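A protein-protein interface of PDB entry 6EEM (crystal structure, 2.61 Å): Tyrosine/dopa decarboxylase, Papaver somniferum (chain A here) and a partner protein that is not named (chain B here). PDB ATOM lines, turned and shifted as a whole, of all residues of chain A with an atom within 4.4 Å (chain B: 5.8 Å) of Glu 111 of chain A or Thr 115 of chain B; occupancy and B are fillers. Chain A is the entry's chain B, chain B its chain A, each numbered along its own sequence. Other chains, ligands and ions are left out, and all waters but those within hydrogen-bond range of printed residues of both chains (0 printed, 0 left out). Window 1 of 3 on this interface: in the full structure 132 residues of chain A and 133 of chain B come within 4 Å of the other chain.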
ATOM      1  N   GLY A 107      14.094 -12.393   3.484  1.00  0.00           N
ATOM      2  CA  GLY A 107      13.534 -11.555   2.439  1.00  0.00           C
ATOM      3  C   GLY A 107      13.642 -10.084   2.778  1.00  0.00           C
ATOM      4  O   GLY A 107      14.039  -9.264   1.943  1.00  0.00           O
ATOM      5  N   PHE A 108      13.290  -9.732   4.015  1.00  0.00           N
ATOM      6  CA  PHE A 108      13.431  -8.352   4.464  1.00  0.00           C
ATOM      7  C   PHE A 108      14.878  -7.879   4.338  1.00  0.00           C
ATOM      8  O   PHE A 108      15.149  -6.777   3.846  1.00  0.00           O
ATOM      9  CB  PHE A 108      12.939  -8.234   5.902  1.00  0.00           C
ATOM     10  CG  PHE A 108      12.994  -6.844   6.445  1.00  0.00           C
ATOM     11  CD1 PHE A 108      11.970  -5.952   6.191  1.00  0.00           C
ATOM     12  CD2 PHE A 108      14.071  -6.427   7.217  1.00  0.00           C
ATOM     13  CE1 PHE A 108      12.022  -4.662   6.691  1.00  0.00           C
ATOM     14  CE2 PHE A 108      14.126  -5.142   7.722  1.00  0.00           C
ATOM     15  CZ  PHE A 108      13.101  -4.258   7.458  1.00  0.00           C
ATOM     16  N   LEU A 109      15.823  -8.706   4.782  1.00  0.00           N
ATOM     17  CA  LEU A 109      17.224  -8.307   4.761  1.00  0.00           C
ATOM     18  C   LEU A 109      17.721  -8.119   3.334  1.00  0.00           C
ATOM     19  O   LEU A 109      18.490  -7.192   3.052  1.00  0.00           O
ATOM     20  CB  LEU A 109      18.069  -9.344   5.498  1.00  0.00           C
ATOM     21  CG  LEU A 109      17.678  -9.546   6.964  1.00  0.00           C
ATOM     22  CD1 LEU A 109      18.383 -10.758   7.545  1.00  0.00           C
ATOM     23  CD2 LEU A 109      17.976  -8.302   7.786  1.00  0.00           C
ATOM     24  N   GLY A 110      17.298  -8.990   2.419  1.00  0.00           N
ATOM     25  CA  GLY A 110      17.680  -8.815   1.027  1.00  0.00           C
ATOM     26  C   GLY A 110      17.109  -7.542   0.437  1.00  0.00           C
ATOM     27  O   GLY A 110      17.805  -6.798  -0.268  1.00  0.00           O
ATOM     28  N   GLU A 111      15.833  -7.270   0.719  1.00  0.00           N
ATOM     29  CA  GLU A 111      15.242  -6.012   0.283  1.00  0.00           C
ATOM     30  C   GLU A 111      16.028  -4.825   0.826  1.00  0.00           C
ATOM     31  O   GLU A 111      16.264  -3.844   0.113  1.00  0.00           O
ATOM     32  CB  GLU A 111      13.784  -5.935   0.730  1.00  0.00           C
ATOM     33  CG  GLU A 111      13.043  -4.753   0.153  1.00  0.00           C
ATOM     34  CD  GLU A 111      12.976  -4.811  -1.356  1.00  0.00           C
ATOM     35  OE1 GLU A 111      13.255  -5.891  -1.921  1.00  0.00           O
ATOM     36  OE2 GLU A 111      12.654  -3.778  -1.977  1.00  0.00           O
ATOM     37  N   MET A 112      16.442  -4.898   2.092  1.00  0.00           N
ATOM     38  CA  MET A 112      17.100  -3.753   2.703  1.00  0.00           C
ATOM     39  C   MET A 112      18.517  -3.579   2.176  1.00  0.00           C
ATOM     40  O   MET A 112      18.981  -2.448   2.038  1.00  0.00           O
ATOM     41  CB  MET A 112      17.078  -3.878   4.226  1.00  0.00           C
ATOM     42  CG  MET A 112      15.681  -3.663   4.841  1.00  0.00           C
ATOM     43  SD  MET A 112      14.734  -2.230   4.214  1.00  0.00           S
ATOM     44  CE  MET A 112      13.869  -2.923   2.799  1.00  0.00           C
ATOM     45  N   LEU A 113      19.205  -4.672   1.843  1.00  0.00           N
ATOM     46  CA  LEU A 113      20.500  -4.555   1.177  1.00  0.00           C
ATOM     47  C   LEU A 113      20.350  -3.929  -0.203  1.00  0.00           C
ATOM     48  O   LEU A 113      21.133  -3.050  -0.591  1.00  0.00           O
ATOM     49  CB  LEU A 113      21.160  -5.929   1.065  1.00  0.00           C
ATOM     50  CG  LEU A 113      21.880  -6.473   2.295  1.00  0.00           C
ATOM     51  CD1 LEU A 113      22.202  -7.948   2.117  1.00  0.00           C
ATOM     52  CD2 LEU A 113      23.143  -5.669   2.533  1.00  0.00           C
ATOM     53  N   SER A 114      19.349  -4.372  -0.962  1.00  0.00           N
ATOM     54  CA  SER A 114      19.093  -3.771  -2.266  1.00  0.00           C
ATOM     55  C   SER A 114      18.809  -2.274  -2.138  1.00  0.00           C
ATOM     56  O   SER A 114      19.389  -1.455  -2.859  1.00  0.00           O
ATOM     57  CB  SER A 114      17.932  -4.497  -2.940  1.00  0.00           C
ATOM     58  OG  SER A 114      17.520  -3.834  -4.117  1.00  0.00           O
ATOM     59  N   THR A 115      17.921  -1.899  -1.217  1.00  0.00           N
ATOM     60  CA  THR A 115      17.611  -0.488  -1.017  1.00  0.00           C
ATOM     61  C   THR A 115      18.810   0.289  -0.480  1.00  0.00           C
ATOM     62  O   THR A 115      18.969   1.478  -0.787  1.00  0.00           O
ATOM     63  CB  THR A 115      16.423  -0.346  -0.073  1.00  0.00           C
ATOM     64  OG1 THR A 115      15.252  -0.836  -0.725  1.00  0.00           O
ATOM     65  CG2 THR A 115      16.211   1.100   0.296  1.00  0.00           C
ATOM     66  N   THR A 326       9.056 -11.616   0.259  1.00  0.00           N
ATOM     67  CA  THR A 326       8.547 -10.270   0.502  1.00  0.00           C
ATOM     68  C   THR A 326       8.180  -9.621  -0.837  1.00  0.00           C
ATOM     69  O   THR A 326       8.626 -10.069  -1.900  1.00  0.00           O
ATOM     70  CB  THR A 326       9.584  -9.445   1.281  1.00  0.00           C
ATOM     71  OG1 THR A 326       9.099  -9.151   2.595  1.00  0.00           O
ATOM     72  CG2 THR A 326       9.960  -8.168   0.546  1.00  0.00           C
ATOM     73  N   ARG A 374      15.073  -2.760 -10.147  1.00  0.00           N
ATOM     74  CA  ARG A 374      15.567  -2.913  -8.793  1.00  0.00           C
ATOM     75  C   ARG A 374      16.388  -4.188  -8.681  1.00  0.00           C
ATOM     76  O   ARG A 374      16.164  -5.161  -9.406  1.00  0.00           O
ATOM     77  CB  ARG A 374      14.413  -2.942  -7.792  1.00  0.00           C
ATOM     78  CG  ARG A 374      13.504  -1.735  -7.881  1.00  0.00           C
ATOM     79  CD  ARG A 374      12.490  -1.734  -6.763  1.00  0.00           C
ATOM     80  NE  ARG A 374      13.131  -1.581  -5.463  1.00  0.00           N
ATOM     81  CZ  ARG A 374      12.477  -1.301  -4.340  1.00  0.00           C
ATOM     82  NH1 ARG A 374      11.158  -1.139  -4.363  1.00  0.00           N
ATOM     83  NH2 ARG A 374      13.146  -1.178  -3.199  1.00  0.00           N
ATOM     84  N   LYS A 379      16.764 -10.367  -2.706  1.00  0.00           N
ATOM     85  CA  LYS A 379      15.746 -11.039  -1.890  1.00  0.00           C
ATOM     86  C   LYS A 379      15.772 -12.546  -2.098  1.00  0.00           C
ATOM     87  O   LYS A 379      15.810 -13.324  -1.134  1.00  0.00           O
ATOM     88  CB  LYS A 379      14.349 -10.513  -2.228  1.00  0.00           C
ATOM     89  CG  LYS A 379      13.953  -9.245  -1.524  1.00  0.00           C
ATOM     90  CD  LYS A 379      12.556  -8.810  -1.941  1.00  0.00           C
ATOM     91  CE  LYS A 379      12.455  -8.655  -3.449  1.00  0.00           C
ATOM     92  NZ  LYS A 379      11.220  -7.924  -3.839  1.00  0.00           N
ATOM     93  N   GLY B 110      11.377   4.709   5.111  1.00  0.00           N
ATOM     94  CA  GLY B 110      10.063   4.479   4.531  1.00  0.00           C
ATOM     95  C   GLY B 110       9.972   3.139   3.826  1.00  0.00           C
ATOM     96  O   GLY B 110       8.986   2.408   3.965  1.00  0.00           O
ATOM     97  N   GLU B 111      11.004   2.801   3.049  1.00  0.00           N
ATOM     98  CA  GLU B 111      11.037   1.489   2.406  1.00  0.00           C
ATOM     99  C   GLU B 111      11.105   0.369   3.443  1.00  0.00           C
ATOM    100  O   GLU B 111      10.491  -0.690   3.270  1.00  0.00           O
ATOM    101  CB  GLU B 111      12.216   1.395   1.439  1.00  0.00           C
ATOM    102  CG  GLU B 111      12.182   0.162   0.539  1.00  0.00           C
ATOM    103  CD  GLU B 111      11.047   0.213  -0.471  1.00  0.00           C
ATOM    104  OE1 GLU B 111      10.472   1.306  -0.663  1.00  0.00           O
ATOM    105  OE2 GLU B 111      10.727  -0.834  -1.072  1.00  0.00           O
ATOM    106  N   MET B 112      11.857   0.582   4.526  1.00  0.00           N
ATOM    107  CA  MET B 112      11.900  -0.399   5.605  1.00  0.00           C
ATOM    108  C   MET B 112      10.506  -0.659   6.149  1.00  0.00           C
ATOM    109  O   MET B 112      10.075  -1.809   6.258  1.00  0.00           O
ATOM    110  CB  MET B 112      12.818   0.082   6.730  1.00  0.00           C
ATOM    111  CG  MET B 112      14.280  -0.168   6.510  1.00  0.00           C
ATOM    112  SD  MET B 112      15.114  -0.642   8.039  1.00  0.00           S
ATOM    113  CE  MET B 112      15.073   0.890   8.960  1.00  0.00           C
ATOM    114  N   LEU B 113       9.798   0.409   6.516  1.00  0.00           N
ATOM    115  CA  LEU B 113       8.446   0.274   7.043  1.00  0.00           C
ATOM    116  C   LEU B 113       7.535  -0.437   6.048  1.00  0.00           C
ATOM    117  O   LEU B 113       6.797  -1.363   6.410  1.00  0.00           O
ATOM    118  CB  LEU B 113       7.891   1.652   7.395  1.00  0.00           C
ATOM    119  CG  LEU B 113       7.975   2.077   8.859  1.00  0.00           C
ATOM    120  CD1 LEU B 113       8.949   1.199   9.606  1.00  0.00           C
ATOM    121  CD2 LEU B 113       8.378   3.536   8.953  1.00  0.00           C
ATOM    122  N   SER B 114       7.564  -0.012   4.788  1.00  0.00           N
ATOM    123  CA  SER B 114       6.750  -0.673   3.777  1.00  0.00           C
ATOM    124  C   SER B 114       7.027  -2.175   3.753  1.00  0.00           C
ATOM    125  O   SER B 114       6.123  -2.994   3.951  1.00  0.00           O
ATOM    126  CB  SER B 114       7.009  -0.040   2.411  1.00  0.00           C
ATOM    127  OG  SER B 114       6.289  -0.704   1.390  1.00  0.00           O
ATOM    128  N   THR B 115       8.290  -2.552   3.538  1.00  0.00           N
ATOM    129  CA  THR B 115       8.647  -3.965   3.440  1.00  0.00           C
ATOM    130  C   THR B 115       8.361  -4.720   4.731  1.00  0.00           C
ATOM    131  O   THR B 115       8.111  -5.931   4.694  1.00  0.00           O
ATOM    132  CB  THR B 115      10.124  -4.097   3.069  1.00  0.00           C
ATOM    133  OG1 THR B 115      10.339  -3.473   1.802  1.00  0.00           O
ATOM    134  CG2 THR B 115      10.535  -5.552   2.984  1.00  0.00           C
ATOM    135  N   GLY B 116       8.397  -4.039   5.872  1.00  0.00           N
ATOM    136  CA  GLY B 116       8.174  -4.698   7.142  1.00  0.00           C
ATOM    137  C   GLY B 116       6.712  -5.002   7.379  1.00  0.00           C
ATOM    138  O   GLY B 116       6.373  -6.051   7.928  1.00  0.00           O
ATOM    139  N   PHE B 117       5.834  -4.080   6.974  1.00  0.00           N
ATOM    140  CA  PHE B 117       4.404  -4.375   6.987  1.00  0.00           C
ATOM    141  C   PHE B 117       4.045  -5.366   5.890  1.00  0.00           C
ATOM    142  O   PHE B 117       3.167  -6.217   6.077  1.00  0.00           O
ATOM    143  CB  PHE B 117       3.602  -3.088   6.828  1.00  0.00           C
ATOM    144  CG  PHE B 117       3.678  -2.182   8.010  1.00  0.00           C
ATOM    145  CD1 PHE B 117       3.578  -2.689   9.293  1.00  0.00           C
ATOM    146  CD2 PHE B 117       3.855  -0.820   7.847  1.00  0.00           C
ATOM    147  CE1 PHE B 117       3.646  -1.857  10.393  1.00  0.00           C
ATOM    148  CE2 PHE B 117       3.926   0.017   8.948  1.00  0.00           C
ATOM    149  CZ  PHE B 117       3.819  -0.504  10.218  1.00  0.00           C
ATOM    150  N   ASN B 118       4.711  -5.265   4.742  1.00  0.00           N
ATOM    151  CA  ASN B 118       4.521  -6.177   3.617  1.00  0.00           C
ATOM    152  C   ASN B 118       3.036  -6.413   3.332  1.00  0.00           C
ATOM    153  O   ASN B 118       2.547  -7.543   3.322  1.00  0.00           O
ATOM    154  CB  ASN B 118       5.251  -7.499   3.868  1.00  0.00           C
ATOM    155  CG  ASN B 118       5.451  -8.313   2.596  1.00  0.00           C
ATOM    156  OD1 ASN B 118       5.663  -7.762   1.516  1.00  0.00           O
ATOM    157  ND2 ASN B 118       5.384  -9.632   2.722  1.00  0.00           N
ATOM    158  N   ARG B 374       3.029  -1.749  -4.170  1.00  0.00           N
ATOM    159  CA  ARG B 374       3.858  -1.544  -2.998  1.00  0.00           C
ATOM    160  C   ARG B 374       3.348  -0.336  -2.227  1.00  0.00           C
ATOM    161  O   ARG B 374       2.864   0.636  -2.816  1.00  0.00           O
ATOM    162  CB  ARG B 374       5.321  -1.350  -3.390  1.00  0.00           C
ATOM    163  CG  ARG B 374       5.887  -2.481  -4.227  1.00  0.00           C
ATOM    164  CD  ARG B 374       7.403  -2.543  -4.135  1.00  0.00           C
ATOM    165  NE  ARG B 374       7.847  -2.784  -2.763  1.00  0.00           N
ATOM    166  CZ  ARG B 374       9.035  -3.282  -2.437  1.00  0.00           C
ATOM    167  NH1 ARG B 374       9.907  -3.612  -3.382  1.00  0.00           N
ATOM    168  NH2 ARG B 374       9.349  -3.464  -1.161  1.00  0.00           N
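The guanidinium group of Arg 374 of chain A lies within salt-bridge range of the side-chain carboxylate of Glu 111 of chain B (3.2 Å).
The guanidinium group (NH1) of Arg 374 of chain B lies within salt-bridge range of the side-chain carboxylate (OE2) of Glu 111 of chain A (3.1 Å).
The guanidinium group (NH1) of Arg 374 of chain A sits close to the guanidinium group (NH1) of Arg 374 of chain B (2.9 Å).
O of Glu 111 of chain B is in hydrogen-bond range of OG1 of Thr 115 of chain B, 3.2 Å away.
OE2 of Glu 111 of chain B is in salt-bridge range of NH2 of Arg 374 of chain B (3.0 Å).
The side-chain hydroxyl (OG1) of Thr 115 of chain B sits at hydrogen-bond distance from the guanidinium group (NH2) of Arg 374 of chain B (3.1 Å).
NH2 of Arg 374 of chain A is in salt-bridge range of OE2 of Glu 111 of chain A, 2.9 Å away.
OE1 of Glu 111 of chain A lies within salt-bridge range of NZ of Lys 379 of chain A.
OG1 of Thr 115 of chain A lies within hydrogen-bond range of NH2 of Arg 374 of chain A (3.3 Å).
CE1 of Phe 108 of chain A touches O of Met 112 of chain B, at 3.5 Å.
CD1 of Phe 108 of chain A touches CG2 of Thr 115 of chain B, at 3.5 Å.
CE1 of Phe 108 of chain A touches N of Gly 116 of chain B, at 3.8 Å.
Glu 111 of chain A touches Glu 111 of chain B (OE2 to OE2, 3.6 Å).
Glu 111 of chain A touches Thr 115 of chain B.
SD of Met 112 of chain A touches CG of Met 112 of chain B, at 3.1 Å.
Thr 115 of chain B touches Met 112 of chain A (OG1 to CE, 3.7 Å).
Glu 111 of chain B touches Thr 115 of chain A.
CG2 of Thr 115 of chain B touches CG2 of Thr 326 of chain A, at 3.6 Å.
OG1 of Thr 326 of chain A touches CG of Asn 118 of chain B, 3.7 Å away.
Of chain B, only Glu 111 (3.6 Å), Thr 115 (3.4 Å) and Arg 374 (3.1 Å) come within 4 Å of Glu 111 of chain A.
Of chain A, only Phe 108, Glu 111, Met 112 and Thr 326 come within 4 Å of Thr 115 of chain B.
Printed residues of chain A within 4 Å of Asn 118 of chain B: Thr 326.
Printed residues of chain A within 4 Å of Glu 111 of chain B: Glu 111 (3.6 Å), Thr 115 (3.5 Å) and Arg 374 (3.2 Å).
Of the printed residues of chain A, Gly 116 of chain B touches Phe 108 (3.8 Å).
Of the printed residues of chain B, Thr 115 of chain A touches Glu 111 (3.5 Å).
The nearest printed residue of chain A that does not touch Thr 115 of chain B is Gly 107 of chain A (5.2 Å).
The nearest printed residue of chain B that does not touch Arg 374 of chain A is Thr 115 of chain B (6.2 Å).
Of the 12 printed residues of chain A, 6 touch a printed residue of chain B.
Hydrophobic or aromatic side chains of chain A that line the printed part of chain B: Phe 108 and Met 112.
Among the printed residues, 13 pairs touch across the chains.
Among the printed residues, Asp or Glu carboxylates within 4 Å of a Lys or Arg side-chain nitrogen of the other chain: Glu 111 of chain A with Arg 374 of chain B and Arg 374 of chain A with Glu 111 of chain B.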
